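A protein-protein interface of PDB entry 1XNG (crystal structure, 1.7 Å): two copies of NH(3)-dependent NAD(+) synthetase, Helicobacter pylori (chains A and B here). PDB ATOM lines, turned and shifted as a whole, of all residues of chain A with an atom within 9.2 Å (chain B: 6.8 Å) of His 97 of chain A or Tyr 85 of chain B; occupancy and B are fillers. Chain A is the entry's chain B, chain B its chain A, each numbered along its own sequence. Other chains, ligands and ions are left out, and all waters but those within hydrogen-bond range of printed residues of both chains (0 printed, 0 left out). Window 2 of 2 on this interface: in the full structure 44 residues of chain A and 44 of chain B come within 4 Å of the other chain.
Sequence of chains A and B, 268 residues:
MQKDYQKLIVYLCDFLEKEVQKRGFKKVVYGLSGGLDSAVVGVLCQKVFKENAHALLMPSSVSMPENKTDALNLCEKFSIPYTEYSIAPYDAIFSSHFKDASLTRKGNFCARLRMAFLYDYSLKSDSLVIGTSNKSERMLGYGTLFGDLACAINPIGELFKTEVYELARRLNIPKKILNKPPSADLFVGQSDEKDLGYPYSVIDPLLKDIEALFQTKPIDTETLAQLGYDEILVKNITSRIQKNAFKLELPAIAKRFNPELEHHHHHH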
ATOM      1  N   TYR A  90      11.091  18.403 -11.408  1.00  0.00           N
ATOM      2  CA  TYR A  90      10.717  18.898 -12.725  1.00  0.00           C
ATOM      3  C   TYR A  90       9.735  17.968 -13.427  1.00  0.00           C
ATOM      4  O   TYR A  90       8.747  18.421 -14.006  1.00  0.00           O
ATOM      5  CB  TYR A  90      11.951  19.084 -13.611  1.00  0.00           C
ATOM      6  CG  TYR A  90      12.987  20.031 -13.057  1.00  0.00           C
ATOM      7  CD1 TYR A  90      14.007  19.574 -12.224  1.00  0.00           C
ATOM      8  CD2 TYR A  90      12.960  21.385 -13.390  1.00  0.00           C
ATOM      9  CE1 TYR A  90      14.978  20.442 -11.742  1.00  0.00           C
ATOM     10  CE2 TYR A  90      13.919  22.257 -12.913  1.00  0.00           C
ATOM     11  CZ  TYR A  90      14.925  21.780 -12.096  1.00  0.00           C
ATOM     12  OH  TYR A  90      15.894  22.640 -11.647  1.00  0.00           O
ATOM     13  N   ASP A  91      10.001  16.667 -13.386  1.00  0.00           N
ATOM     14  CA  ASP A  91       9.098  15.741 -14.046  1.00  0.00           C
ATOM     15  C   ASP A  91       7.766  15.684 -13.309  1.00  0.00           C
ATOM     16  O   ASP A  91       6.748  15.312 -13.884  1.00  0.00           O
ATOM     17  CB  ASP A  91       9.734  14.344 -14.176  1.00  0.00           C
ATOM     18  CG  ASP A  91       9.910  13.632 -12.845  1.00  0.00           C
ATOM     19  OD1 ASP A  91      11.036  13.162 -12.578  1.00  0.00           O
ATOM     20  OD2 ASP A  91       8.931  13.518 -12.075  1.00  0.00           O
ATOM     21  N   ALA A  92       7.768  16.074 -12.037  1.00  0.00           N
ATOM     22  CA  ALA A  92       6.542  16.084 -11.249  1.00  0.00           C
ATOM     23  C   ALA A  92       5.588  17.130 -11.824  1.00  0.00           C
ATOM     24  O   ALA A  92       4.375  16.919 -11.870  1.00  0.00           O
ATOM     25  CB  ALA A  92       6.856  16.399  -9.789  1.00  0.00           C
ATOM     26  N   ILE A  93       6.135  18.262 -12.262  1.00  0.00           N
ATOM     27  CA  ILE A  93       5.306  19.307 -12.846  1.00  0.00           C
ATOM     28  C   ILE A  93       4.756  18.803 -14.177  1.00  0.00           C
ATOM     29  O   ILE A  93       3.576  18.974 -14.482  1.00  0.00           O
ATOM     30  CB  ILE A  93       6.111  20.599 -13.086  1.00  0.00           C
ATOM     31  CG1 ILE A  93       6.670  21.113 -11.758  1.00  0.00           C
ATOM     32  CG2 ILE A  93       5.224  21.641 -13.733  1.00  0.00           C
ATOM     33  CD1 ILE A  93       7.427  22.414 -11.868  1.00  0.00           C
ATOM     34  N   PHE A  94       5.617  18.165 -14.964  1.00  0.00           N
ATOM     35  CA  PHE A  94       5.204  17.634 -16.257  1.00  0.00           C
ATOM     36  C   PHE A  94       4.055  16.637 -16.097  1.00  0.00           C
ATOM     37  O   PHE A  94       3.084  16.672 -16.857  1.00  0.00           O
ATOM     38  CB  PHE A  94       6.395  16.963 -16.952  1.00  0.00           C
ATOM     39  CG  PHE A  94       6.107  16.515 -18.360  1.00  0.00           C
ATOM     40  CD1 PHE A  94       5.481  15.298 -18.604  1.00  0.00           C
ATOM     41  CD2 PHE A  94       6.449  17.321 -19.442  1.00  0.00           C
ATOM     42  CE1 PHE A  94       5.200  14.891 -19.908  1.00  0.00           C
ATOM     43  CE2 PHE A  94       6.171  16.921 -20.747  1.00  0.00           C
ATOM     44  CZ  PHE A  94       5.545  15.704 -20.979  1.00  0.00           C
ATOM     45  N   SER A  95       4.167  15.758 -15.104  1.00  0.00           N
ATOM     46  CA  SER A  95       3.136  14.752 -14.842  1.00  0.00           C
ATOM     47  C   SER A  95       1.825  15.406 -14.440  1.00  0.00           C
ATOM     48  O   SER A  95       0.743  14.918 -14.766  1.00  0.00           O
ATOM     49  CB  SER A  95       3.578  13.807 -13.723  1.00  0.00           C
ATOM     50  OG  SER A  95       4.694  13.034 -14.116  1.00  0.00           O
ATOM     51  N   SER A  96       1.930  16.509 -13.712  1.00  0.00           N
ATOM     52  CA  SER A  96       0.750  17.229 -13.272  1.00  0.00           C
ATOM     53  C   SER A  96       0.060  17.921 -14.439  1.00  0.00           C
ATOM     54  O   SER A  96      -1.169  17.949 -14.515  1.00  0.00           O
ATOM     55  CB  SER A  96       1.133  18.267 -12.221  1.00  0.00           C
ATOM     56  OG  SER A  96      -0.003  19.022 -11.846  1.00  0.00           O
ATOM     57  N   HIS A  97       0.857  18.478 -15.349  1.00  0.00           N
ATOM     58  CA  HIS A  97       0.330  19.190 -16.508  1.00  0.00           C
ATOM     59  C   HIS A  97      -0.138  18.258 -17.622  1.00  0.00           C
ATOM     60  O   HIS A  97      -1.065  18.586 -18.362  1.00  0.00           O
ATOM     61  CB  HIS A  97       1.388  20.150 -17.065  1.00  0.00           C
ATOM     62  CG  HIS A  97       1.654  21.338 -16.191  1.00  0.00           C
ATOM     63  ND1 HIS A  97       1.180  21.441 -14.902  1.00  0.00           N
ATOM     64  CD2 HIS A  97       2.375  22.464 -16.418  1.00  0.00           C
ATOM     65  CE1 HIS A  97       1.597  22.578 -14.370  1.00  0.00           C
ATOM     66  NE2 HIS A  97       2.322  23.217 -15.267  1.00  0.00           N
ATOM     67  N   PHE A  98       0.510  17.104 -17.743  1.00  0.00           N
ATOM     68  CA  PHE A  98       0.152  16.131 -18.771  1.00  0.00           C
ATOM     69  C   PHE A  98       0.040  14.746 -18.138  1.00  0.00           C
ATOM     70  O   PHE A  98       0.896  13.882 -18.332  1.00  0.00           O
ATOM     71  CB  PHE A  98       1.210  16.113 -19.879  1.00  0.00           C
ATOM     72  CG  PHE A  98       1.574  17.478 -20.389  1.00  0.00           C
ATOM     73  CD1 PHE A  98       2.662  18.162 -19.859  1.00  0.00           C
ATOM     74  CD2 PHE A  98       0.821  18.086 -21.388  1.00  0.00           C
ATOM     75  CE1 PHE A  98       2.997  19.437 -20.311  1.00  0.00           C
ATOM     76  CE2 PHE A  98       1.146  19.362 -21.850  1.00  0.00           C
ATOM     77  CZ  PHE A  98       2.237  20.039 -21.311  1.00  0.00           C
ATOM     78  N   LYS A  99      -1.029  14.543 -17.376  1.00  0.00           N
ATOM     79  CA  LYS A  99      -1.243  13.276 -16.693  1.00  0.00           C
ATOM     80  C   LYS A  99      -1.413  12.102 -17.642  1.00  0.00           C
ATOM     81  O   LYS A  99      -0.957  10.997 -17.349  1.00  0.00           O
ATOM     82  CB  LYS A  99      -2.463  13.373 -15.777  1.00  0.00           C
ATOM     83  CG  LYS A  99      -2.362  14.482 -14.742  1.00  0.00           C
ATOM     84  CD  LYS A  99      -3.487  14.388 -13.729  1.00  0.00           C
ATOM     85  CE  LYS A  99      -3.348  15.449 -12.652  1.00  0.00           C
ATOM     86  NZ  LYS A  99      -4.383  15.281 -11.592  1.00  0.00           N
ATOM     87  N   ASP A 100      -2.061  12.339 -18.778  1.00  0.00           N
ATOM     88  CA  ASP A 100      -2.295  11.280 -19.754  1.00  0.00           C
ATOM     89  C   ASP A 100      -1.229  11.187 -20.844  1.00  0.00           C
ATOM     90  O   ASP A 100      -1.430  10.525 -21.863  1.00  0.00           O
ATOM     91  CB  ASP A 100      -3.677  11.456 -20.393  1.00  0.00           C
ATOM     92  CG  ASP A 100      -4.805  11.376 -19.375  1.00  0.00           C
ATOM     93  OD1 ASP A 100      -4.882  10.358 -18.656  1.00  0.00           O
ATOM     94  OD2 ASP A 100      -5.612  12.328 -19.290  1.00  0.00           O
ATOM     95  N   ALA A 101      -0.094  11.846 -20.629  1.00  0.00           N
ATOM     96  CA  ALA A 101       0.990  11.803 -21.602  1.00  0.00           C
ATOM     97  C   ALA A 101       1.482  10.363 -21.716  1.00  0.00           C
ATOM     98  O   ALA A 101       1.510   9.629 -20.730  1.00  0.00           O
ATOM     99  CB  ALA A 101       2.129  12.710 -21.159  1.00  0.00           C
ATOM    100  N   ARG A 105       6.520  10.026 -24.247  1.00  0.00           N
ATOM    101  CA  ARG A 105       6.622  11.473 -24.079  1.00  0.00           C
ATOM    102  C   ARG A 105       7.247  11.815 -22.727  1.00  0.00           C
ATOM    103  O   ARG A 105       8.141  12.658 -22.643  1.00  0.00           O
ATOM    104  CB  ARG A 105       5.249  12.153 -24.187  1.00  0.00           C
ATOM    105  CG  ARG A 105       4.774  12.457 -25.603  1.00  0.00           C
ATOM    106  CD  ARG A 105       3.809  13.648 -25.583  1.00  0.00           C
ATOM    107  NE  ARG A 105       2.479  13.297 -25.099  1.00  0.00           N
ATOM    108  CZ  ARG A 105       1.645  14.148 -24.508  1.00  0.00           C
ATOM    109  NH1 ARG A 105       1.997  15.412 -24.308  1.00  0.00           N
ATOM    110  NH2 ARG A 105       0.449  13.732 -24.131  1.00  0.00           N
ATOM    111  N   LYS A 106       6.782  11.161 -21.664  1.00  0.00           N
ATOM    112  CA  LYS A 106       7.319  11.431 -20.332  1.00  0.00           C
ATOM    113  C   LYS A 106       8.804  11.104 -20.254  1.00  0.00           C
ATOM    114  O   LYS A 106       9.590  11.851 -19.670  1.00  0.00           O
ATOM    115  CB  LYS A 106       6.571  10.625 -19.267  1.00  0.00           C
ATOM    116  CG  LYS A 106       5.112  11.015 -19.084  1.00  0.00           C
ATOM    117  CD  LYS A 106       4.434  10.128 -18.036  1.00  0.00           C
ATOM    118  CE  LYS A 106       3.010  10.591 -17.765  1.00  0.00           C
ATOM    119  NZ  LYS A 106       2.354   9.792 -16.691  1.00  0.00           N
ATOM    120  N   PHE A 109      10.957  13.677 -22.054  1.00  0.00           N
ATOM    121  CA  PHE A 109      11.126  14.895 -21.280  1.00  0.00           C
ATOM    122  C   PHE A 109      12.245  14.701 -20.259  1.00  0.00           C
ATOM    123  O   PHE A 109      13.086  15.575 -20.101  1.00  0.00           O
ATOM    124  CB  PHE A 109       9.826  15.287 -20.574  1.00  0.00           C
ATOM    125  CG  PHE A 109       9.903  16.616 -19.871  1.00  0.00           C
ATOM    126  CD1 PHE A 109      10.143  17.780 -20.591  1.00  0.00           C
ATOM    127  CD2 PHE A 109       9.760  16.699 -18.489  1.00  0.00           C
ATOM    128  CE1 PHE A 109      10.236  19.011 -19.947  1.00  0.00           C
ATOM    129  CE2 PHE A 109       9.853  17.930 -17.837  1.00  0.00           C
ATOM    130  CZ  PHE A 109      10.093  19.085 -18.567  1.00  0.00           C
ATOM    131  N   LEU B  56       3.590  27.829 -30.820  1.00  0.00           N
ATOM    132  CA  LEU B  56       3.648  27.522 -29.401  1.00  0.00           C
ATOM    133  C   LEU B  56       4.338  28.676 -28.683  1.00  0.00           C
ATOM    134  O   LEU B  56       5.508  28.963 -28.937  1.00  0.00           O
ATOM    135  CB  LEU B  56       4.435  26.228 -29.168  1.00  0.00           C
ATOM    136  CG  LEU B  56       4.004  25.299 -28.024  1.00  0.00           C
ATOM    137  CD1 LEU B  56       5.080  24.250 -27.802  1.00  0.00           C
ATOM    138  CD2 LEU B  56       3.763  26.076 -26.758  1.00  0.00           C
ATOM    139  N   LEU B  57       3.601  29.344 -27.798  1.00  0.00           N
ATOM    140  CA  LEU B  57       4.132  30.459 -27.023  1.00  0.00           C
ATOM    141  C   LEU B  57       4.489  29.923 -25.634  1.00  0.00           C
ATOM    142  O   LEU B  57       3.643  29.352 -24.939  1.00  0.00           O
ATOM    143  CB  LEU B  57       3.089  31.586 -26.938  1.00  0.00           C
ATOM    144  CG  LEU B  57       2.717  32.313 -28.246  1.00  0.00           C
ATOM    145  CD1 LEU B  57       1.995  31.375 -29.199  1.00  0.00           C
ATOM    146  CD2 LEU B  57       1.833  33.517 -27.930  1.00  0.00           C
ATOM    147  N   MET B  58       5.750  30.106 -25.241  1.00  0.00           N
ATOM    148  CA  MET B  58       6.250  29.599 -23.968  1.00  0.00           C
ATOM    149  C   MET B  58       6.976  30.640 -23.132  1.00  0.00           C
ATOM    150  O   MET B  58       8.198  30.598 -22.989  1.00  0.00           O
ATOM    151  CB  MET B  58       7.186  28.414 -24.234  1.00  0.00           C
ATOM    152  CG  MET B  58       6.521  27.312 -25.045  1.00  0.00           C
ATOM    153  SD  MET B  58       7.676  26.064 -25.631  1.00  0.00           S
ATOM    154  CE  MET B  58       8.247  26.813 -27.144  1.00  0.00           C
ATOM    155  N   PRO B  59       6.226  31.592 -22.555  1.00  0.00           N
ATOM    156  CA  PRO B  59       6.884  32.611 -21.739  1.00  0.00           C
ATOM    157  C   PRO B  59       7.510  32.011 -20.480  1.00  0.00           C
ATOM    158  O   PRO B  59       7.037  30.999 -19.950  1.00  0.00           O
ATOM    159  CB  PRO B  59       5.746  33.570 -21.411  1.00  0.00           C
ATOM    160  CG  PRO B  59       4.575  32.643 -21.286  1.00  0.00           C
ATOM    161  CD  PRO B  59       4.760  31.721 -22.486  1.00  0.00           C
ATOM    162  N   SER B  60       8.576  32.646 -20.008  1.00  0.00           N
ATOM    163  CA  SER B  60       9.284  32.209 -18.810  1.00  0.00           C
ATOM    164  C   SER B  60       8.963  33.196 -17.697  1.00  0.00           C
ATOM    165  O   SER B  60       8.054  34.016 -17.834  1.00  0.00           O
ATOM    166  CB  SER B  60      10.791  32.225 -19.051  1.00  0.00           C
ATOM    167  OG  SER B  60      11.229  33.551 -19.304  1.00  0.00           O
ATOM    168  N   THR B  83      -1.012  27.885 -29.020  1.00  0.00           N
ATOM    169  CA  THR B  83      -1.178  27.357 -27.671  1.00  0.00           C
ATOM    170  C   THR B  83      -0.176  28.065 -26.773  1.00  0.00           C
ATOM    171  O   THR B  83       0.999  28.200 -27.121  1.00  0.00           O
ATOM    172  CB  THR B  83      -0.903  25.838 -27.588  1.00  0.00           C
ATOM    173  OG1 THR B  83      -1.884  25.125 -28.349  1.00  0.00           O
ATOM    174  CG2 THR B  83      -0.968  25.367 -26.141  1.00  0.00           C
ATOM    175  N   GLU B  84      -0.639  28.536 -25.622  1.00  0.00           N
ATOM    176  CA  GLU B  84       0.252  29.209 -24.695  1.00  0.00           C
ATOM    177  C   GLU B  84       0.577  28.239 -23.565  1.00  0.00           C
ATOM    178  O   GLU B  84      -0.322  27.680 -22.936  1.00  0.00           O
ATOM    179  CB  GLU B  84      -0.402  30.481 -24.132  1.00  0.00           C
ATOM    180  CG  GLU B  84       0.600  31.435 -23.482  1.00  0.00           C
ATOM    181  CD  GLU B  84      -0.046  32.632 -22.810  1.00  0.00           C
ATOM    182  OE1 GLU B  84      -0.950  33.249 -23.417  1.00  0.00           O
ATOM    183  OE2 GLU B  84       0.367  32.961 -21.674  1.00  0.00           O
ATOM    184  N   TYR B  85       1.866  28.026 -23.319  1.00  0.00           N
ATOM    185  CA  TYR B  85       2.295  27.127 -22.258  1.00  0.00           C
ATOM    186  C   TYR B  85       3.480  27.727 -21.515  1.00  0.00           C
ATOM    187  O   TYR B  85       4.584  27.821 -22.047  1.00  0.00           O
ATOM    188  CB  TYR B  85       2.678  25.757 -22.824  1.00  0.00           C
ATOM    189  CG  TYR B  85       3.062  24.761 -21.750  1.00  0.00           C
ATOM    190  CD1 TYR B  85       2.116  24.285 -20.840  1.00  0.00           C
ATOM    191  CD2 TYR B  85       4.383  24.336 -21.606  1.00  0.00           C
ATOM    192  CE1 TYR B  85       2.479  23.417 -19.808  1.00  0.00           C
ATOM    193  CE2 TYR B  85       4.755  23.470 -20.580  1.00  0.00           C
ATOM    194  CZ  TYR B  85       3.800  23.017 -19.686  1.00  0.00           C
ATOM    195  OH  TYR B  85       4.171  22.180 -18.661  1.00  0.00           O
ATOM    196  N   SER B  86       3.245  28.128 -20.273  1.00  0.00           N
ATOM    197  CA  SER B  86       4.300  28.730 -19.475  1.00  0.00           C
ATOM    198  C   SER B  86       5.334  27.744 -18.952  1.00  0.00           C
ATOM    199  O   SER B  86       4.998  26.652 -18.490  1.00  0.00           O
ATOM    200  CB  SER B  86       3.701  29.489 -18.291  1.00  0.00           C
ATOM    201  OG  SER B  86       4.727  29.894 -17.404  1.00  0.00           O
ATOM    202  N   ILE B  87       6.603  28.134 -19.027  1.00  0.00           N
ATOM    203  CA  ILE B  87       7.673  27.291 -18.520  1.00  0.00           C
ATOM    204  C   ILE B  87       8.202  27.893 -17.217  1.00  0.00           C
ATOM    205  O   ILE B  87       9.203  27.443 -16.666  1.00  0.00           O
ATOM    206  CB  ILE B  87       8.829  27.153 -19.539  1.00  0.00           C
ATOM    207  CG1 ILE B  87       9.361  28.532 -19.937  1.00  0.00           C
ATOM    208  CG2 ILE B  87       8.336  26.393 -20.766  1.00  0.00           C
ATOM    209  CD1 ILE B  87      10.636  28.487 -20.768  1.00  0.00           C
ATOM    210  N   ALA B  88       7.506  28.915 -16.725  1.00  0.00           N
ATOM    211  CA  ALA B  88       7.891  29.584 -15.489  1.00  0.00           C
ATOM    212  C   ALA B  88       7.982  28.613 -14.305  1.00  0.00           C
ATOM    213  O   ALA B  88       8.925  28.673 -13.514  1.00  0.00           O
ATOM    214  CB  ALA B  88       6.902  30.716 -15.183  1.00  0.00           C
ATOM    215  N   PRO B  89       7.006  27.699 -14.166  1.00  0.00           N
ATOM    216  CA  PRO B  89       7.093  26.768 -13.037  1.00  0.00           C
ATOM    217  C   PRO B  89       8.391  25.967 -13.053  1.00  0.00           C
ATOM    218  O   PRO B  89       8.882  25.551 -12.005  1.00  0.00           O
ATOM    219  CB  PRO B  89       5.851  25.891 -13.213  1.00  0.00           C
ATOM    220  CG  PRO B  89       5.610  25.934 -14.689  1.00  0.00           C
ATOM    221  CD  PRO B  89       5.841  27.390 -15.008  1.00  0.00           C
ATOM    222  N   TYR B  90       8.954  25.758 -14.243  1.00  0.00           N
ATOM    223  CA  TYR B  90      10.198  25.011 -14.349  1.00  0.00           C
ATOM    224  C   TYR B  90      11.427  25.881 -14.099  1.00  0.00           C
ATOM    225  O   TYR B  90      12.355  25.451 -13.421  1.00  0.00           O
ATOM    226  CB  TYR B  90      10.333  24.341 -15.722  1.00  0.00           C
ATOM    227  CG  TYR B  90       9.186  23.433 -16.092  1.00  0.00           C
ATOM    228  CD1 TYR B  90       8.053  23.936 -16.719  1.00  0.00           C
ATOM    229  CD2 TYR B  90       9.240  22.061 -15.828  1.00  0.00           C
ATOM    230  CE1 TYR B  90       7.002  23.105 -17.081  1.00  0.00           C
ATOM    231  CE2 TYR B  90       8.190  21.220 -16.184  1.00  0.00           C
ATOM    232  CZ  TYR B  90       7.079  21.751 -16.813  1.00  0.00           C
ATOM    233  OH  TYR B  90       6.046  20.933 -17.196  1.00  0.00           O
ATOM    234  N   PHE B 117       9.527  21.112 -24.932  1.00  0.00           N
ATOM    235  CA  PHE B 117       8.088  21.179 -25.117  1.00  0.00           C
ATOM    236  C   PHE B 117       7.696  21.251 -26.584  1.00  0.00           C
ATOM    237  O   PHE B 117       6.622  20.794 -26.959  1.00  0.00           O
ATOM    238  CB  PHE B 117       7.489  22.331 -24.309  1.00  0.00           C
ATOM    239  CG  PHE B 117       7.523  22.088 -22.831  1.00  0.00           C
ATOM    240  CD1 PHE B 117       8.322  22.865 -22.002  1.00  0.00           C
ATOM    241  CD2 PHE B 117       6.805  21.031 -22.273  1.00  0.00           C
ATOM    242  CE1 PHE B 117       8.410  22.594 -20.638  1.00  0.00           C
ATOM    243  CE2 PHE B 117       6.886  20.750 -20.909  1.00  0.00           C
ATOM    244  CZ  PHE B 117       7.693  21.533 -20.092  1.00  0.00           C
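The backbone carbonyl oxygen (O) of Leu 57 of chain B lies within hydrogen-bond range of the backbone NH (N) of Tyr 85 of chain B, 2.7 Å away. The side-chain hydroxyl of Tyr 85 of chain B sits at hydrogen-bond distance from the side-chain hydroxyl of Tyr 90 of chain B, 2.7 Å away. A ring nitrogen (ND1) of His 97 of chain A lies within hydrogen-bond range of the backbone carbonyl oxygen (O) of Ile 93 of chain A, at 3.5 Å.
Tyr 90 of chain B touches Tyr 90 of chain A. Ile 93 of chain A touches Pro 89 of chain B (CD1 to O, 3.5 Å). CG2 of Ile 93 of chain A touches CZ of Tyr 90 of chain B (3.6 Å). Tyr 90 of chain B touches Phe 94 of chain A. CE2 of Phe 117 of chain B touches CD2 of Phe 94 of chain A (3.8 Å). CD2 of His 97 of chain A touches OH of Tyr 85 of chain B, at 2.9 Å. OH of Tyr 85 of chain B touches CE1 of Phe 98 of chain A, 3.4 Å away. Tyr 90 of chain B touches Phe 109 of chain A. CZ of Phe 117 of chain B touches CE1 of Phe 109 of chain A, at 3.6 Å.
Of chain B, only Tyr 85 (2.9 Å) comes within 4 Å of His 97 of chain A. Tyr 85 of chain B touches two residues of chain A. No residue of chain A comes within 4 Å of Ser 86 of chain B. Printed residues of chain B within 4 Å of Phe 94 of chain A: Tyr 90 and Phe 117. Of the printed residues of chain B, Ile 93 of chain A touches Pro 89 (3.5 Å) and Tyr 90 (3.6 Å). Printed residues of chain B within 4 Å of Phe 109 of chain A: Tyr 90 (3.7 Å) and Phe 117 (3.6 Å). Printed residues of chain B within 4 Å of Tyr 90 of chain A: Tyr 90 (3.6 Å). Of the printed residues of chain A, Pro 89 of chain B touches Ile 93. The nearest residue of chain B that does not touch His 97 of chain A is Tyr 90 of chain B (4.1 Å).
Hydrophobic or aromatic side chains of chain A that line the printed part of chain B: Tyr 90, Ile 93, Phe 94, His 97, Phe 98 and Phe 109. Printed residues of chain B that touch a printed residue of chain A: Tyr 85, Pro 89, Tyr 90 and Phe 117. Hydrophobic or aromatic side chains of chain B within 4 Å of the printed part of chain A: Tyr 85, Tyr 90 and Phe 117. Among the printed residues, no Asp or Glu carboxylate lies within 4 Å of a Lys or Arg side-chain nitrogen of the other chain.
Tyr 90 of chain B touches its own counterpart, Tyr 90 of chain A. Position printed for both chains: 90.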
